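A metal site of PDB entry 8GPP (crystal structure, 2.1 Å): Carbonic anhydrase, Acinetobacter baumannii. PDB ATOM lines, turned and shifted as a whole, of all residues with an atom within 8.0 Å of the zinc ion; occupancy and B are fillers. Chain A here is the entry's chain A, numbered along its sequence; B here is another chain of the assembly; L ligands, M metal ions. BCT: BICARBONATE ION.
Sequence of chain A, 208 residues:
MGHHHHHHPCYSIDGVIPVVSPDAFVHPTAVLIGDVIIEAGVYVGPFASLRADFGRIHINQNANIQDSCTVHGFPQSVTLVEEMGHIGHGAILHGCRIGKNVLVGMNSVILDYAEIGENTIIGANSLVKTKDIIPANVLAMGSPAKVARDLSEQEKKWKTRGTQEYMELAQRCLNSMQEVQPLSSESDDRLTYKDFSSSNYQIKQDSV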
ATOM      1  N   ARG A  51      19.888 -22.851   6.505  1.00  0.00           N
ATOM      2  CA  ARG A  51      20.603 -24.054   6.115  1.00  0.00           C
ATOM      3  C   ARG A  51      21.216 -23.802   4.740  1.00  0.00           C
ATOM      4  O   ARG A  51      20.545 -23.959   3.721  1.00  0.00           O
ATOM      5  CB  ARG A  51      19.683 -25.269   6.114  1.00  0.00           C
ATOM      6  CG  ARG A  51      20.444 -26.578   5.915  1.00  0.00           C
ATOM      7  CD  ARG A  51      19.835 -27.716   6.696  1.00  0.00           C
ATOM      8  NE  ARG A  51      18.519 -28.088   6.171  1.00  0.00           N
ATOM      9  CZ  ARG A  51      18.328 -28.875   5.132  1.00  0.00           C
ATOM     10  NH1 ARG A  51      19.356 -29.361   4.431  1.00  0.00           N
ATOM     11  NH2 ARG A  51      17.087 -29.203   4.784  1.00  0.00           N
ATOM     12  N   ASP A  53      23.661 -25.574   3.097  1.00  0.00           N
ATOM     13  CA  ASP A  53      24.497 -26.745   2.837  1.00  0.00           C
ATOM     14  C   ASP A  53      24.477 -27.149   1.366  1.00  0.00           C
ATOM     15  O   ASP A  53      25.209 -28.061   0.976  1.00  0.00           O
ATOM     16  CB  ASP A  53      24.087 -27.941   3.728  1.00  0.00           C
ATOM     17  CG  ASP A  53      22.589 -28.160   3.772  1.00  0.00           C
ATOM     18  OD1 ASP A  53      21.896 -27.597   2.886  1.00  0.00           O
ATOM     19  OD2 ASP A  53      22.105 -28.910   4.659  1.00  0.00           O
ATOM     20  N   PHE A  54      23.641 -26.504   0.561  1.00  0.00           N
ATOM     21  CA  PHE A  54      23.640 -26.689  -0.892  1.00  0.00           C
ATOM     22  C   PHE A  54      24.007 -25.429  -1.657  1.00  0.00           C
ATOM     23  O   PHE A  54      24.626 -25.512  -2.716  1.00  0.00           O
ATOM     24  CB  PHE A  54      22.258 -27.149  -1.359  1.00  0.00           C
ATOM     25  CG  PHE A  54      21.922 -28.556  -1.005  1.00  0.00           C
ATOM     26  CD1 PHE A  54      22.925 -29.515  -0.867  1.00  0.00           C
ATOM     27  CD2 PHE A  54      20.613 -28.927  -0.805  1.00  0.00           C
ATOM     28  CE1 PHE A  54      22.603 -30.840  -0.545  1.00  0.00           C
ATOM     29  CE2 PHE A  54      20.298 -30.233  -0.491  1.00  0.00           C
ATOM     30  CZ  PHE A  54      21.291 -31.189  -0.357  1.00  0.00           C
ATOM     31  N   THR A  70      12.501 -21.198   8.043  1.00  0.00           N
ATOM     32  CA  THR A  70      13.519 -21.990   7.377  1.00  0.00           C
ATOM     33  C   THR A  70      13.959 -21.308   6.090  1.00  0.00           C
ATOM     34  O   THR A  70      13.132 -20.915   5.265  1.00  0.00           O
ATOM     35  CB  THR A  70      13.007 -23.417   7.117  1.00  0.00           C
ATOM     36  OG1 THR A  70      12.746 -24.030   8.385  1.00  0.00           O
ATOM     37  CG2 THR A  70      14.042 -24.262   6.348  1.00  0.00           C
ATOM     38  N   VAL A  71      15.271 -21.174   5.922  1.00  0.00           N
ATOM     39  CA  VAL A  71      15.863 -20.660   4.702  1.00  0.00           C
ATOM     40  C   VAL A  71      16.749 -21.747   4.123  1.00  0.00           C
ATOM     41  O   VAL A  71      17.708 -22.170   4.770  1.00  0.00           O
ATOM     42  CB  VAL A  71      16.661 -19.370   4.939  1.00  0.00           C
ATOM     43  CG1 VAL A  71      17.033 -18.765   3.593  1.00  0.00           C
ATOM     44  CG2 VAL A  71      15.857 -18.369   5.766  1.00  0.00           C
ATOM     45  N   HIS A  72      16.442 -22.177   2.911  1.00  0.00           N
ATOM     46  CA  HIS A  72      17.211 -23.231   2.251  1.00  0.00           C
ATOM     47  C   HIS A  72      17.230 -22.938   0.754  1.00  0.00           C
ATOM     48  O   HIS A  72      16.638 -21.962   0.273  1.00  0.00           O
ATOM     49  CB  HIS A  72      16.646 -24.621   2.536  1.00  0.00           C
ATOM     50  CG  HIS A  72      17.597 -25.744   2.244  1.00  0.00           C
ATOM     51  ND1 HIS A  72      17.293 -26.777   1.386  1.00  0.00           N
ATOM     52  CD2 HIS A  72      18.852 -25.975   2.687  1.00  0.00           C
ATOM     53  CE1 HIS A  72      18.314 -27.606   1.314  1.00  0.00           C
ATOM     54  NE2 HIS A  72      19.281 -27.141   2.091  1.00  0.00           N
ATOM     55  N   GLY A  73      17.916 -23.789  -0.001  1.00  0.00           N
ATOM     56  CA  GLY A  73      17.991 -23.531  -1.427  1.00  0.00           C
ATOM     57  C   GLY A  73      18.564 -24.699  -2.194  1.00  0.00           C
ATOM     58  O   GLY A  73      19.057 -25.673  -1.611  1.00  0.00           O
ATOM     59  N   PHE A  74      18.504 -24.575  -3.515  1.00  0.00           N
ATOM     60  CA  PHE A  74      19.028 -25.594  -4.409  1.00  0.00           C
ATOM     61  C   PHE A  74      20.545 -25.652  -4.333  1.00  0.00           C
ATOM     62  O   PHE A  74      21.190 -24.720  -3.858  1.00  0.00           O
ATOM     63  CB  PHE A  74      18.666 -25.286  -5.849  1.00  0.00           C
ATOM     64  CG  PHE A  74      17.223 -25.456  -6.186  1.00  0.00           C
ATOM     65  CD1 PHE A  74      16.474 -26.483  -5.630  1.00  0.00           C
ATOM     66  CD2 PHE A  74      16.625 -24.617  -7.121  1.00  0.00           C
ATOM     67  CE1 PHE A  74      15.127 -26.646  -5.964  1.00  0.00           C
ATOM     68  CE2 PHE A  74      15.291 -24.781  -7.462  1.00  0.00           C
ATOM     69  CZ  PHE A  74      14.536 -25.800  -6.885  1.00  0.00           C
ATOM     70  N   PRO A  75      21.130 -26.738  -4.816  1.00  0.00           N
ATOM     71  CA  PRO A  75      22.580 -26.741  -5.016  1.00  0.00           C
ATOM     72  C   PRO A  75      22.958 -25.544  -5.875  1.00  0.00           C
ATOM     73  O   PRO A  75      22.296 -25.238  -6.880  1.00  0.00           O
ATOM     74  CB  PRO A  75      22.832 -28.064  -5.734  1.00  0.00           C
ATOM     75  CG  PRO A  75      21.687 -28.956  -5.300  1.00  0.00           C
ATOM     76  CD  PRO A  75      20.504 -28.044  -5.121  1.00  0.00           C
ATOM     77  N   ILE A  92       8.845 -20.081   5.087  1.00  0.00           N
ATOM     78  CA  ILE A  92       9.897 -20.905   4.495  1.00  0.00           C
ATOM     79  C   ILE A  92      10.380 -20.238   3.201  1.00  0.00           C
ATOM     80  O   ILE A  92       9.582 -19.935   2.308  1.00  0.00           O
ATOM     81  CB  ILE A  92       9.384 -22.335   4.266  1.00  0.00           C
ATOM     82  CG1 ILE A  92       9.013 -22.953   5.634  1.00  0.00           C
ATOM     83  CG2 ILE A  92      10.398 -23.187   3.489  1.00  0.00           C
ATOM     84  CD1 ILE A  92       8.063 -24.113   5.529  1.00  0.00           C
ATOM     85  N   LEU A  93      11.684 -19.940   3.134  1.00  0.00           N
ATOM     86  CA  LEU A  93      12.306 -19.295   1.984  1.00  0.00           C
ATOM     87  C   LEU A  93      13.185 -20.321   1.299  1.00  0.00           C
ATOM     88  O   LEU A  93      14.155 -20.810   1.883  1.00  0.00           O
ATOM     89  CB  LEU A  93      13.151 -18.089   2.383  1.00  0.00           C
ATOM     90  CG  LEU A  93      12.534 -16.959   3.196  1.00  0.00           C
ATOM     91  CD1 LEU A  93      13.476 -15.792   3.235  1.00  0.00           C
ATOM     92  CD2 LEU A  93      11.162 -16.541   2.658  1.00  0.00           C
ATOM     93  N   HIS A  94      12.879 -20.626   0.051  1.00  0.00           N
ATOM     94  CA  HIS A  94      13.615 -21.648  -0.683  1.00  0.00           C
ATOM     95  C   HIS A  94      14.120 -21.073  -1.995  1.00  0.00           C
ATOM     96  O   HIS A  94      13.345 -20.959  -2.953  1.00  0.00           O
ATOM     97  CB  HIS A  94      12.771 -22.881  -0.913  1.00  0.00           C
ATOM     98  CG  HIS A  94      13.590 -24.109  -1.087  1.00  0.00           C
ATOM     99  ND1 HIS A  94      14.016 -24.545  -2.316  1.00  0.00           N
ATOM    100  CD2 HIS A  94      14.120 -24.956  -0.176  1.00  0.00           C
ATOM    101  CE1 HIS A  94      14.750 -25.630  -2.174  1.00  0.00           C
ATOM    102  NE2 HIS A  94      14.838 -25.897  -0.882  1.00  0.00           N
ATOM    103  N   GLY A  95      15.406 -20.746  -2.024  1.00  0.00           N
ATOM    104  CA  GLY A  95      16.046 -20.279  -3.251  1.00  0.00           C
ATOM    105  C   GLY A  95      15.385 -19.111  -3.937  1.00  0.00           C
ATOM    106  O   GLY A  95      15.326 -19.076  -5.177  1.00  0.00           O
ATOM    107  N   ASP A 112      11.441 -21.557  -5.267  1.00  0.00           N
ATOM    108  CA  ASP A 112      12.729 -21.275  -5.882  1.00  0.00           C
ATOM    109  C   ASP A 112      12.608 -20.345  -7.069  1.00  0.00           C
ATOM    110  O   ASP A 112      11.704 -20.489  -7.904  1.00  0.00           O
ATOM    111  CB  ASP A 112      13.380 -22.577  -6.320  1.00  0.00           C
ATOM    112  CG  ASP A 112      13.543 -23.530  -5.173  1.00  0.00           C
ATOM    113  OD1 ASP A 112      12.580 -24.263  -4.848  1.00  0.00           O
ATOM    114  OD2 ASP A 112      14.653 -23.520  -4.600  1.00  0.00           O
ATOM    115  N   ASN B  64      14.524 -38.607   4.126  1.00  0.00           N
ATOM    116  CA  ASN B  64      14.992 -37.394   4.785  1.00  0.00           C
ATOM    117  C   ASN B  64      13.824 -36.648   5.396  1.00  0.00           C
ATOM    118  O   ASN B  64      12.743 -36.556   4.785  1.00  0.00           O
ATOM    119  CB  ASN B  64      15.744 -36.481   3.820  1.00  0.00           C
ATOM    120  CG  ASN B  64      14.888 -36.033   2.669  1.00  0.00           C
ATOM    121  OD1 ASN B  64      14.117 -35.070   2.794  1.00  0.00           O
ATOM    122  ND2 ASN B  64      15.035 -36.715   1.542  1.00  0.00           N
ATOM    123  N   GLN B  66      13.041 -32.893   6.968  1.00  0.00           N
ATOM    124  CA  GLN B  66      13.677 -31.591   6.873  1.00  0.00           C
ATOM    125  C   GLN B  66      13.313 -30.670   8.031  1.00  0.00           C
ATOM    126  O   GLN B  66      12.661 -31.072   9.013  1.00  0.00           O
ATOM    127  CB  GLN B  66      13.365 -30.994   5.518  1.00  0.00           C
ATOM    128  CG  GLN B  66      14.155 -31.706   4.435  1.00  0.00           C
ATOM    129  CD  GLN B  66      13.726 -31.303   3.050  1.00  0.00           C
ATOM    130  OE1 GLN B  66      13.323 -30.162   2.815  1.00  0.00           O
ATOM    131  NE2 GLN B  66      13.814 -32.239   2.123  1.00  0.00           N
ATOM    132  N   ASP B  67      13.723 -29.407   7.918  1.00  0.00           N
ATOM    133  CA  ASP B  67      13.778 -28.510   9.064  1.00  0.00           C
ATOM    134  C   ASP B  67      12.386 -28.265   9.614  1.00  0.00           C
ATOM    135  O   ASP B  67      11.431 -28.035   8.864  1.00  0.00           O
ATOM    136  CB  ASP B  67      14.410 -27.177   8.651  1.00  0.00           C
ATOM    137  CG  ASP B  67      15.570 -27.361   7.682  1.00  0.00           C
ATOM    138  OD1 ASP B  67      16.734 -27.107   8.063  1.00  0.00           O
ATOM    139  OD2 ASP B  67      15.312 -27.805   6.540  1.00  0.00           O
ATOM    140  N   HIS B  86      10.663 -38.205   1.201  1.00  0.00           N
ATOM    141  CA  HIS B  86      11.343 -36.908   1.100  1.00  0.00           C
ATOM    142  C   HIS B  86      10.373 -35.881   1.678  1.00  0.00           C
ATOM    143  O   HIS B  86       9.399 -35.496   1.023  1.00  0.00           O
ATOM    144  CB  HIS B  86      11.680 -36.641  -0.371  1.00  0.00           C
ATOM    145  CG  HIS B  86      12.586 -35.473  -0.600  1.00  0.00           C
ATOM    146  ND1 HIS B  86      13.899 -35.631  -1.004  1.00  0.00           N
ATOM    147  CD2 HIS B  86      12.366 -34.143  -0.529  1.00  0.00           C
ATOM    148  CE1 HIS B  86      14.444 -34.431  -1.168  1.00  0.00           C
ATOM    149  NE2 HIS B  86      13.533 -33.526  -0.883  1.00  0.00           N
ATOM    150  N   ILE B  87      10.602 -35.505   2.934  1.00  0.00           N
ATOM    151  CA  ILE B  87       9.637 -34.731   3.714  1.00  0.00           C
ATOM    152  C   ILE B  87      10.134 -33.293   3.778  1.00  0.00           C
ATOM    153  O   ILE B  87      11.106 -32.995   4.486  1.00  0.00           O
ATOM    154  CB  ILE B  87       9.473 -35.329   5.113  1.00  0.00           C
ATOM    155  CG1 ILE B  87       9.369 -36.866   5.012  1.00  0.00           C
ATOM    156  CG2 ILE B  87       8.278 -34.682   5.848  1.00  0.00           C
ATOM    157  CD1 ILE B  87       8.135 -37.351   4.288  1.00  0.00           C
ATOM    158  N   GLY B  88       9.458 -32.405   3.062  1.00  0.00           N
ATOM    159  CA  GLY B  88       9.944 -31.048   2.928  1.00  0.00           C
ATOM    160  C   GLY B  88       9.798 -30.217   4.190  1.00  0.00           C
ATOM    161  O   GLY B  88       8.986 -30.487   5.079  1.00  0.00           O
ATOM    162  N   HIS B  89      10.606 -29.143   4.230  1.00  0.00           N
ATOM    163  CA  HIS B  89      10.607 -28.173   5.318  1.00  0.00           C
ATOM    164  C   HIS B  89       9.219 -27.899   5.871  1.00  0.00           C
ATOM    165  O   HIS B  89       8.310 -27.493   5.134  1.00  0.00           O
ATOM    166  CB  HIS B  89      11.202 -26.857   4.817  1.00  0.00           C
ATOM    167  CG  HIS B  89      12.467 -27.014   4.056  1.00  0.00           C
ATOM    168  ND1 HIS B  89      13.675 -27.296   4.670  1.00  0.00           N
ATOM    169  CD2 HIS B  89      12.736 -26.914   2.733  1.00  0.00           C
ATOM    170  CE1 HIS B  89      14.621 -27.385   3.747  1.00  0.00           C
ATOM    171  NE2 HIS B  89      14.073 -27.138   2.568  1.00  0.00           N
ATOM    172  N   MET B 106       6.861 -28.743   1.155  1.00  0.00           N
ATOM    173  CA  MET B 106       7.073 -27.976   2.371  1.00  0.00           C
ATOM    174  C   MET B 106       5.766 -27.459   2.932  1.00  0.00           C
ATOM    175  O   MET B 106       4.845 -27.062   2.191  1.00  0.00           O
ATOM    176  CB  MET B 106       8.000 -26.789   2.119  1.00  0.00           C
ATOM    177  CG  MET B 106       8.889 -27.009   0.957  1.00  0.00           C
ATOM    178  SD  MET B 106       9.810 -25.521   0.526  1.00  0.00           S
ATOM    179  CE  MET B 106      10.817 -26.227  -0.809  1.00  0.00           C
ATOM    180  N   TYR B 166      20.017 -35.565  -0.827  1.00  0.00           N
ATOM    181  CA  TYR B 166      19.879 -35.625   0.629  1.00  0.00           C
ATOM    182  C   TYR B 166      20.588 -36.846   1.181  1.00  0.00           C
ATOM    183  O   TYR B 166      21.147 -36.804   2.283  1.00  0.00           O
ATOM    184  CB  TYR B 166      18.416 -35.641   1.046  1.00  0.00           C
ATOM    185  CG  TYR B 166      17.887 -34.264   1.382  1.00  0.00           C
ATOM    186  CD1 TYR B 166      17.425 -33.416   0.369  1.00  0.00           C
ATOM    187  CD2 TYR B 166      17.886 -33.792   2.700  1.00  0.00           C
ATOM    188  CE1 TYR B 166      16.957 -32.155   0.657  1.00  0.00           C
ATOM    189  CE2 TYR B 166      17.407 -32.520   2.996  1.00  0.00           C
ATOM    190  CZ  TYR B 166      16.967 -31.704   1.967  1.00  0.00           C
ATOM    191  OH  TYR B 166      16.492 -30.448   2.211  1.00  0.00           O
HETATM  192  C   BCT L   1      13.324 -29.907  -0.389  1.00  0.00           C
HETATM  193  O1  BCT L   1      14.484 -29.547  -0.164  1.00  0.00           O
HETATM  194  O2  BCT L   1      12.204 -29.733   0.211  1.00  0.00           O
HETATM  195  O3  BCT L   1      13.157 -30.692  -1.590  1.00  0.00           O
HETATM  196 ZN    ZN M   1      15.248 -27.472   0.705  1.00  0.00          ZN
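A ring nitrogen (ND1) of His 94 is in hydrogen-bond range of the side-chain carboxylate (OD2) of Asp 112 (2.6 Å).
The guanidinium group of Arg 51 lies within hydrogen-bond range of a ring nitrogen (NE2) of His 72 (3.2 Å).
A ring nitrogen (ND1) of His 89 of chain B sits at hydrogen-bond distance from the side-chain carboxylate (OD2) of Asp 67 of chain B, 2.5 Å away.
The backbone carbonyl oxygen (O) of Leu 93 lies within hydrogen-bond range of the backbone NH (N) of His 72.
NE2 of His 86 of chain B lies within hydrogen-bond range of NE2 of Gln 66 of chain B (3.3 Å).
OH of Tyr 166 of chain B is in hydrogen-bond range of NH2 of Arg 51, 2.9 Å away.
The side-chain hydroxyl (OH) of Tyr 166 of chain B sits close to the side-chain amide nitrogen (NE2) of Gln 66 of chain B, at 3.2 Å.
The backbone carbonyl oxygen (O) of Ile 87 of chain B lies within hydrogen-bond range of the backbone NH (N) of Gln 66 of chain B (3.1 Å).
Gln 66 of chain B touches the zinc ion.
OH of Tyr 166 of chain B touches the zinc ion, at 3.6 Å.
Within 4 Å of the zinc ion: His 72, His 94, Gln 66 of chain B, His 89 of chain B and Tyr 166 of chain B.
NE2 of His 89 of chain B binds the zinc ion (2.2 Å).
ND1 of His 72 is bound to the zinc ion, at 2.3 Å.
A ring nitrogen (NE2) of His 94 binds the zinc ion, at 2.3 Å.
The zinc ion is bound by an oxygen (O1) of the ligand (2.4 Å).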
